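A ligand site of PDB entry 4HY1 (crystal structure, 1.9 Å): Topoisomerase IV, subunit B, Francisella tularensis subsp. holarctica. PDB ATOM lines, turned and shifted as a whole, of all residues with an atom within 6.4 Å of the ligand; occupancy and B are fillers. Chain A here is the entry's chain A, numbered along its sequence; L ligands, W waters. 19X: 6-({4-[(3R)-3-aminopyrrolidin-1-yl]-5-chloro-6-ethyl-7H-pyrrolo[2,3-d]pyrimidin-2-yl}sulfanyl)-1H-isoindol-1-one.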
ATOM      1  N   GLU A  37      18.105   4.809  -6.308  1.00  0.00           N
ATOM      2  CA  GLU A  37      17.067   4.756  -7.371  1.00  0.00           C
ATOM      3  C   GLU A  37      15.682   4.850  -6.720  1.00  0.00           C
ATOM      4  O   GLU A  37      14.835   5.545  -7.236  1.00  0.00           O
ATOM      5  CB  GLU A  37      17.167   3.474  -8.223  1.00  0.00           C
ATOM      6  CG  GLU A  37      16.116   3.292  -9.320  1.00  0.00           C
ATOM      7  CD  GLU A  37      16.030   4.472 -10.331  1.00  0.00           C
ATOM      8  OE1 GLU A  37      17.071   5.055 -10.674  1.00  0.00           O
ATOM      9  OE2 GLU A  37      14.907   4.781 -10.798  1.00  0.00           O
ATOM     10  N   ILE A  38      15.425   4.096  -5.619  1.00  0.00           N
ATOM     11  CA  ILE A  38      14.093   4.124  -5.028  1.00  0.00           C
ATOM     12  C   ILE A  38      13.878   5.533  -4.473  1.00  0.00           C
ATOM     13  O   ILE A  38      12.790   6.096  -4.602  1.00  0.00           O
ATOM     14  CB  ILE A  38      13.905   3.134  -3.812  1.00  0.00           C
ATOM     15  CG1 ILE A  38      14.103   1.696  -4.246  1.00  0.00           C
ATOM     16  CG2 ILE A  38      12.506   3.281  -3.204  1.00  0.00           C
ATOM     17  CD1 ILE A  38      13.263   1.248  -5.433  1.00  0.00           C
ATOM     18  N   ILE A  39      14.901   6.085  -3.820  1.00  0.00           N
ATOM     19  CA  ILE A  39      14.777   7.428  -3.239  1.00  0.00           C
ATOM     20  C   ILE A  39      14.452   8.469  -4.336  1.00  0.00           C
ATOM     21  O   ILE A  39      13.614   9.340  -4.140  1.00  0.00           O
ATOM     22  CB  ILE A  39      16.052   7.844  -2.498  1.00  0.00           C
ATOM     23  CG1 ILE A  39      16.229   7.002  -1.212  1.00  0.00           C
ATOM     24  CG2 ILE A  39      15.959   9.335  -2.152  1.00  0.00           C
ATOM     25  CD1 ILE A  39      17.674   7.027  -0.696  1.00  0.00           C
ATOM     26  N   ASN A  41      12.766   8.108  -7.016  1.00  0.00           N
ATOM     27  CA  ASN A  41      11.348   8.013  -7.347  1.00  0.00           C
ATOM     28  C   ASN A  41      10.433   8.642  -6.293  1.00  0.00           C
ATOM     29  O   ASN A  41       9.424   9.239  -6.670  1.00  0.00           O
ATOM     30  CB  ASN A  41      10.971   6.556  -7.593  1.00  0.00           C
ATOM     31  CG  ASN A  41      11.521   6.062  -8.929  1.00  0.00           C
ATOM     32  OD1 ASN A  41      10.850   6.145  -9.952  1.00  0.00           O
ATOM     33  ND2 ASN A  41      12.767   5.573  -8.919  1.00  0.00           N
ATOM     34  N   SER A  42      10.736   8.501  -4.999  1.00  0.00           N
ATOM     35  CA  SER A  42       9.942   9.200  -3.977  1.00  0.00           C
ATOM     36  C   SER A  42      10.208  10.704  -4.156  1.00  0.00           C
ATOM     37  O   SER A  42       9.289  11.490  -3.977  1.00  0.00           O
ATOM     38  CB  SER A  42      10.336   8.807  -2.538  1.00  0.00           C
ATOM     39  OG  SER A  42      10.069   7.422  -2.329  1.00  0.00           O
ATOM     40  N   ASP A  44      10.631  12.396  -6.786  1.00  0.00           N
ATOM     41  CA  ASP A  44       9.810  12.905  -7.869  1.00  0.00           C
ATOM     42  C   ASP A  44       8.420  13.259  -7.314  1.00  0.00           C
ATOM     43  O   ASP A  44       7.843  14.276  -7.698  1.00  0.00           O
ATOM     44  CB  ASP A  44       9.691  11.909  -9.034  1.00  0.00           C
ATOM     45  CG  ASP A  44       9.037  12.528 -10.250  1.00  0.00           C
ATOM     46  OD1 ASP A  44       9.732  13.289 -10.958  1.00  0.00           O
ATOM     47  OD2 ASP A  44       7.804  12.316 -10.480  1.00  0.00           O
ATOM     48  N   GLU A  45       7.885  12.465  -6.382  1.00  0.00           N
ATOM     49  CA  GLU A  45       6.621  12.904  -5.693  1.00  0.00           C
ATOM     50  C   GLU A  45       6.730  14.222  -4.911  1.00  0.00           C
ATOM     51  O   GLU A  45       5.788  15.027  -4.936  1.00  0.00           O
ATOM     52  CB  GLU A  45       6.009  11.808  -4.803  1.00  0.00           C
ATOM     53  CG  GLU A  45       5.372  10.731  -5.615  1.00  0.00           C
ATOM     54  CD  GLU A  45       4.148  11.261  -6.290  1.00  0.00           C
ATOM     55  OE1 GLU A  45       3.124  11.431  -5.589  1.00  0.00           O
ATOM     56  OE2 GLU A  45       4.252  11.610  -7.500  1.00  0.00           O
ATOM     57  N   VAL A  66      12.318   1.929   1.935  1.00  0.00           N
ATOM     58  CA  VAL A  66      12.050   3.359   1.690  1.00  0.00           C
ATOM     59  C   VAL A  66      10.541   3.612   1.671  1.00  0.00           C
ATOM     60  O   VAL A  66       9.756   2.911   0.996  1.00  0.00           O
ATOM     61  CB  VAL A  66      12.659   3.834   0.367  1.00  0.00           C
ATOM     62  CG1 VAL A  66      12.431   5.368   0.166  1.00  0.00           C
ATOM     63  CG2 VAL A  66      14.158   3.516   0.320  1.00  0.00           C
ATOM     64  N   ALA A  67      10.150   4.658   2.371  1.00  0.00           N
ATOM     65  CA  ALA A  67       8.731   4.998   2.410  1.00  0.00           C
ATOM     66  C   ALA A  67       8.535   6.507   2.251  1.00  0.00           C
ATOM     67  O   ALA A  67       9.327   7.288   2.729  1.00  0.00           O
ATOM     68  CB  ALA A  67       8.134   4.556   3.742  1.00  0.00           C
ATOM     69  N   ASP A  68       7.468   6.871   1.548  1.00  0.00           N
ATOM     70  CA  ASP A  68       7.100   8.268   1.330  1.00  0.00           C
ATOM     71  C   ASP A  68       5.615   8.507   1.622  1.00  0.00           C
ATOM     72  O   ASP A  68       4.857   7.547   1.823  1.00  0.00           O
ATOM     73  CB  ASP A  68       7.546   8.743  -0.066  1.00  0.00           C
ATOM     74  CG  ASP A  68       6.752   8.118  -1.236  1.00  0.00           C
ATOM     75  OD1 ASP A  68       5.510   8.132  -1.206  1.00  0.00           O
ATOM     76  OD2 ASP A  68       7.374   7.629  -2.207  1.00  0.00           O
ATOM     77  N   GLY A  70       3.756  10.355  -0.641  1.00  0.00           N
ATOM     78  CA  GLY A  70       3.284  10.756  -1.953  1.00  0.00           C
ATOM     79  C   GLY A  70       1.878  10.216  -2.243  1.00  0.00           C
ATOM     80  O   GLY A  70       1.206   9.686  -1.328  1.00  0.00           O
ATOM     81  N   ARG A  71       1.478  10.261  -3.503  1.00  0.00           N
ATOM     82  CA  ARG A  71       0.076   9.929  -3.877  1.00  0.00           C
ATOM     83  C   ARG A  71      -0.220   8.432  -3.756  1.00  0.00           C
ATOM     84  O   ARG A  71      -1.391   8.027  -3.698  1.00  0.00           O
ATOM     85  CB  ARG A  71      -0.191  10.389  -5.317  1.00  0.00           C
ATOM     86  CG  ARG A  71      -0.423  11.890  -5.431  1.00  0.00           C
ATOM     87  CD  ARG A  71      -0.474  12.313  -6.899  1.00  0.00           C
ATOM     88  NE  ARG A  71       0.862  12.303  -7.497  1.00  0.00           N
ATOM     89  CZ  ARG A  71       1.129  12.609  -8.783  1.00  0.00           C
ATOM     90  NH1 ARG A  71       0.148  12.932  -9.638  1.00  0.00           N
ATOM     91  NH2 ARG A  71       2.381  12.574  -9.231  1.00  0.00           N
ATOM     92  N   GLY A  72       0.855   7.636  -3.771  1.00  0.00           N
ATOM     93  CA  GLY A  72       0.786   6.169  -3.787  1.00  0.00           C
ATOM     94  C   GLY A  72       0.877   5.700  -5.229  1.00  0.00           C
ATOM     95  O   GLY A  72       0.131   6.181  -6.099  1.00  0.00           O
ATOM     96  N   MET A  73       1.812   4.779  -5.502  1.00  0.00           N
ATOM     97  CA  MET A  73       2.008   4.251  -6.859  1.00  0.00           C
ATOM     98  C   MET A  73       0.692   3.738  -7.441  1.00  0.00           C
ATOM     99  O   MET A  73      -0.106   3.116  -6.713  1.00  0.00           O
ATOM    100  CB  MET A  73       3.026   3.113  -6.866  1.00  0.00           C
ATOM    101  CG  MET A  73       4.426   3.524  -6.515  1.00  0.00           C
ATOM    102  SD  MET A  73       5.691   2.284  -6.895  1.00  0.00           S
ATOM    103  CE  MET A  73       4.992   1.496  -8.368  1.00  0.00           C
ATOM    104  N   PRO A  74       0.435   3.997  -8.739  1.00  0.00           N
ATOM    105  CA  PRO A  74      -0.914   3.702  -9.279  1.00  0.00           C
ATOM    106  C   PRO A  74      -1.148   2.185  -9.299  1.00  0.00           C
ATOM    107  O   PRO A  74      -0.207   1.425  -9.513  1.00  0.00           O
ATOM    108  CB  PRO A  74      -0.875   4.300 -10.716  1.00  0.00           C
ATOM    109  CG  PRO A  74       0.231   5.310 -10.673  1.00  0.00           C
ATOM    110  CD  PRO A  74       1.269   4.752  -9.711  1.00  0.00           C
ATOM    111  N   ILE A  89       5.162  -1.157 -13.725  1.00  0.00           N
ATOM    112  CA  ILE A  89       6.338  -0.373 -13.355  1.00  0.00           C
ATOM    113  C   ILE A  89       7.494  -1.212 -12.830  1.00  0.00           C
ATOM    114  O   ILE A  89       8.678  -1.001 -13.180  1.00  0.00           O
ATOM    115  CB  ILE A  89       5.921   0.683 -12.307  1.00  0.00           C
ATOM    116  CG1 ILE A  89       5.133   1.826 -12.991  1.00  0.00           C
ATOM    117  CG2 ILE A  89       7.158   1.177 -11.556  1.00  0.00           C
ATOM    118  CD1 ILE A  89       4.204   2.576 -12.033  1.00  0.00           C
ATOM    119  N   MET A  90       7.160  -2.202 -11.984  1.00  0.00           N
ATOM    120  CA  MET A  90       8.175  -3.047 -11.353  1.00  0.00           C
ATOM    121  C   MET A  90       8.751  -4.185 -12.163  1.00  0.00           C
ATOM    122  O   MET A  90       9.860  -4.593 -11.891  1.00  0.00           O
ATOM    123  CB  MET A  90       7.651  -3.656 -10.046  1.00  0.00           C
ATOM    124  CG  MET A  90       7.518  -2.659  -8.920  1.00  0.00           C
ATOM    125  SD  MET A  90       9.170  -2.166  -8.329  1.00  0.00           S
ATOM    126  CE  MET A  90       8.637  -0.611  -7.662  1.00  0.00           C
ATOM    127  N   VAL A 115      12.733   1.989 -11.531  1.00  0.00           N
ATOM    128  CA  VAL A 115      12.791   1.184 -10.309  1.00  0.00           C
ATOM    129  C   VAL A 115      12.707  -0.280 -10.570  1.00  0.00           C
ATOM    130  O   VAL A 115      13.036  -1.056  -9.702  1.00  0.00           O
ATOM    131  CB  VAL A 115      11.598   1.508  -9.347  1.00  0.00           C
ATOM    132  CG1 VAL A 115      11.858   2.822  -8.660  1.00  0.00           C
ATOM    133  CG2 VAL A 115      10.241   1.505 -10.110  1.00  0.00           C
ATOM    134  N   ARG A 131      -3.608   4.341  -0.901  1.00  0.00           N
ATOM    135  CA  ARG A 131      -4.251   5.137  -1.946  1.00  0.00           C
ATOM    136  C   ARG A 131      -5.753   4.905  -1.890  1.00  0.00           C
ATOM    137  O   ARG A 131      -6.170   3.766  -1.850  1.00  0.00           O
ATOM    138  CB  ARG A 131      -3.768   4.581  -3.257  1.00  0.00           C
ATOM    139  CG  ARG A 131      -3.641   5.612  -4.305  1.00  0.00           C
ATOM    140  CD  ARG A 131      -3.315   4.911  -5.605  1.00  0.00           C
ATOM    141  NE  ARG A 131      -4.003   5.669  -6.604  1.00  0.00           N
ATOM    142  CZ  ARG A 131      -3.474   6.654  -7.310  1.00  0.00           C
ATOM    143  NH1 ARG A 131      -2.189   6.960  -7.176  1.00  0.00           N
ATOM    144  NH2 ARG A 131      -4.220   7.283  -8.190  1.00  0.00           N
ATOM    145  N   GLY A 161       0.711   7.106   0.319  1.00  0.00           N
ATOM    146  CA  GLY A 161       2.141   6.980   0.063  1.00  0.00           C
ATOM    147  C   GLY A 161       2.543   5.603  -0.403  1.00  0.00           C
ATOM    148  O   GLY A 161       1.716   4.731  -0.640  1.00  0.00           O
ATOM    149  N   THR A 162       3.834   5.391  -0.530  1.00  0.00           N
ATOM    150  CA  THR A 162       4.361   4.164  -1.074  1.00  0.00           C
ATOM    151  C   THR A 162       5.514   3.758  -0.189  1.00  0.00           C
ATOM    152  O   THR A 162       6.292   4.598   0.233  1.00  0.00           O
ATOM    153  CB  THR A 162       4.849   4.385  -2.516  1.00  0.00           C
ATOM    154  OG1 THR A 162       3.768   4.930  -3.300  1.00  0.00           O
ATOM    155  CG2 THR A 162       5.411   3.119  -3.145  1.00  0.00           C
ATOM    156  N   LYS A 163       5.609   2.469   0.096  1.00  0.00           N
ATOM    157  CA  LYS A 163       6.659   1.894   0.930  1.00  0.00           C
ATOM    158  C   LYS A 163       7.184   0.650   0.186  1.00  0.00           C
ATOM    159  O   LYS A 163       6.410  -0.268  -0.149  1.00  0.00           O
ATOM    160  CB  LYS A 163       6.081   1.527   2.299  1.00  0.00           C
ATOM    161  CG  LYS A 163       7.072   0.810   3.213  1.00  0.00           C
ATOM    162  CD  LYS A 163       6.447   0.462   4.578  1.00  0.00           C
ATOM    163  CE  LYS A 163       6.462   1.672   5.483  1.00  0.00           C
ATOM    164  NZ  LYS A 163       5.602   1.529   6.693  1.00  0.00           N
ATOM    165  N   ILE A 164       8.490   0.640  -0.069  1.00  0.00           N
ATOM    166  CA  ILE A 164       9.139  -0.432  -0.768  1.00  0.00           C
ATOM    167  C   ILE A 164      10.240  -1.031   0.091  1.00  0.00           C
ATOM    168  O   ILE A 164      11.135  -0.330   0.563  1.00  0.00           O
ATOM    169  CB  ILE A 164       9.688   0.043  -2.128  1.00  0.00           C
ATOM    170  CG1 ILE A 164       8.519   0.373  -3.084  1.00  0.00           C
ATOM    171  CG2 ILE A 164      10.664  -0.991  -2.726  1.00  0.00           C
ATOM    172  CD1 ILE A 164       8.972   1.103  -4.341  1.00  0.00           C
HETATM  173  O29 19X L   1      -1.770   8.997  -9.420  1.00  0.00           O
HETATM  174  C28 19X L   1      -0.714   9.193 -10.139  1.00  0.00           C
HETATM  175  C22 19X L   1       0.606   9.003  -9.547  1.00  0.00           C
HETATM  176  C21 19X L   1       1.065   8.601  -8.307  1.00  0.00           C
HETATM  177  N27 19X L   1      -0.694   9.578 -11.455  1.00  0.00           N
HETATM  178  C26 19X L   1       0.733   9.660 -11.889  1.00  0.00           C
HETATM  179  C23 19X L   1       1.485   9.300 -10.678  1.00  0.00           C
HETATM  180  C24 19X L   1       2.847   9.208 -10.515  1.00  0.00           C
HETATM  181  C25 19X L   1       3.314   8.840  -9.233  1.00  0.00           C
HETATM  182  C20 19X L   1       2.459   8.525  -8.168  1.00  0.00           C
HETATM  183  S19 19X L   1       3.057   8.111  -6.629  1.00  0.00           S
HETATM  184  C10 19X L   1       4.526   7.256  -6.769  1.00  0.00           C
HETATM  185  N11 19X L   1       5.259   7.200  -5.631  1.00  0.00           N
HETATM  186  C2  19X L   1       6.365   6.449  -5.560  1.00  0.00           C
HETATM  187  N9  19X L   1       4.857   6.652  -7.915  1.00  0.00           N
HETATM  188  C8  19X L   1       5.954   5.897  -8.045  1.00  0.00           C
HETATM  189  N13 19X L   1       6.278   5.491  -9.312  1.00  0.00           N
HETATM  190  C17 19X L   1       7.662   5.167  -9.724  1.00  0.00           C
HETATM  191  C16 19X L   1       7.757   5.700 -11.157  1.00  0.00           C
HETATM  192  N18 19X L   1       8.298   7.086 -11.216  1.00  0.00           N
HETATM  193  C15 19X L   1       6.302   5.741 -11.614  1.00  0.00           C
HETATM  194  C14 19X L   1       5.364   5.733 -10.410  1.00  0.00           C
HETATM  195  C3  19X L   1       6.778   5.766  -6.814  1.00  0.00           C
HETATM  196  C4  19X L   1       7.958   5.109  -6.283  1.00  0.00           C
HETATM  197 CL1  19X L   1       8.959   3.913  -7.164  1.00  0.00          CL
HETATM  198  C5  19X L   1       8.216   5.379  -4.870  1.00  0.00           C
HETATM  199  N1  19X L   1       7.204   6.178  -4.529  1.00  0.00           N
HETATM  200  C6  19X L   1       9.405   4.895  -4.059  1.00  0.00           C
HETATM  201  C7  19X L   1       8.981   4.343  -2.711  1.00  0.00           C
HETATM  202  O   HOH W   1       3.922   7.658  -3.255  1.00  0.00           O
HETATM  203  O   HOH W   2      10.370   9.024 -11.176  1.00  0.00           O
HETATM  204  O   HOH W   3       7.625   8.517  -8.609  1.00  0.00           O
HETATM  205  O   HOH W   4      -2.954  11.425 -12.332  1.00  0.00           O
HETATM  206  O   HOH W   5       6.166  10.758  -9.081  1.00  0.00           O
HETATM  207  O   HOH W   6       6.094   9.455 -11.507  1.00  0.00           O
HETATM  208  O   HOH W   7       8.432   7.781 -13.690  1.00  0.00           O
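A nitrogen (N1) of the ligand lies within hydrogen-bond range of the side-chain carboxylate of Asp 68 (2.7 Å). A nitrogen (N18) of the ligand is in hydrogen-bond range of the side-chain amide oxygen of Asn 41 (3.0 Å). NH1 of Arg 131 lies within hydrogen-bond range of O29 of the ligand, at 3.1 Å. The backbone NH (N) of Met 73 lies close to a sulfur (S19) of the ligand (3.7 Å). A sulfur (S19) of the ligand lies close to the backbone NH (N) of Gly 72 (3.6 Å).
The side-chain carboxylate (OD1) of Asp 68 lies within hydrogen-bond range of the backbone NH (N) of Gly 70 (2.9 Å). The guanidinium group (NH1) of Arg 131 sits at hydrogen-bond distance from the backbone carbonyl oxygen (O) of Gly 72 (2.7 Å). The side-chain hydroxyl (OG1) of Thr 162 lies within hydrogen-bond range of the backbone NH (N) of Met 73 (2.9 Å). NH2 of Arg 71 is in salt-bridge range of OE2 of Glu 45 (2.7 Å). ND2 of Asn 41 is in hydrogen-bond range of O of Glu 37 (2.7 Å). OD2 of Asp 68 lies within hydrogen-bond range of OG of Ser 42. The backbone carbonyl oxygen (O) of Thr 162 sits at hydrogen-bond distance from the backbone NH (N) of Asp 68, 2.9 Å away. The backbone NH (N) of Ile 164 sits at hydrogen-bond distance from the backbone carbonyl oxygen (O) of Val 66, at 2.8 Å.
The side-chain carboxylate (OE1) of Glu 45 sits close to a sulfur (S19) of the ligand (3.5 Å). Merely in contact with the ligand: Ser 42, Val 115, Thr 162, Ile 38, Ile 164, Arg 71, Ile 89 and Pro 74. Within 4 Å of the ligand: Ile 38, Asn 41, Ser 42, Glu 45, Asp 68, Arg 71, Gly 72, Met 73, Pro 74, Ile 89, Val 115, Arg 131, Thr 162 and Ile 164. Along chain A the residues within 4 Å of the ligand span positions 38 to 164.
Water W1 lies within hydrogen-bond range of OD1 of Asp 68 (2.6 Å), OG1 of Thr 162 (2.7 Å), N11 of the ligand (2.8 Å) and N of Gly 72 (3.1 Å). Water W2 lies within hydrogen-bond range of a nitrogen (N18) of the ligand (2.8 Å) and the side-chain amide oxygen of Asn 41 (3.2 Å). Water W3 lies within hydrogen-bond range of O of Asn 41 (2.7 Å) and N18 of the ligand (3.0 Å). Water W6 lies within hydrogen-bond range of a nitrogen (N18) of the ligand (3.2 Å) and the side-chain carboxylate (OD2) of Asp 44 (3.5 Å). Water W5 lies within hydrogen-bond range of OE2 of Glu 45 and OD2 of Asp 44.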
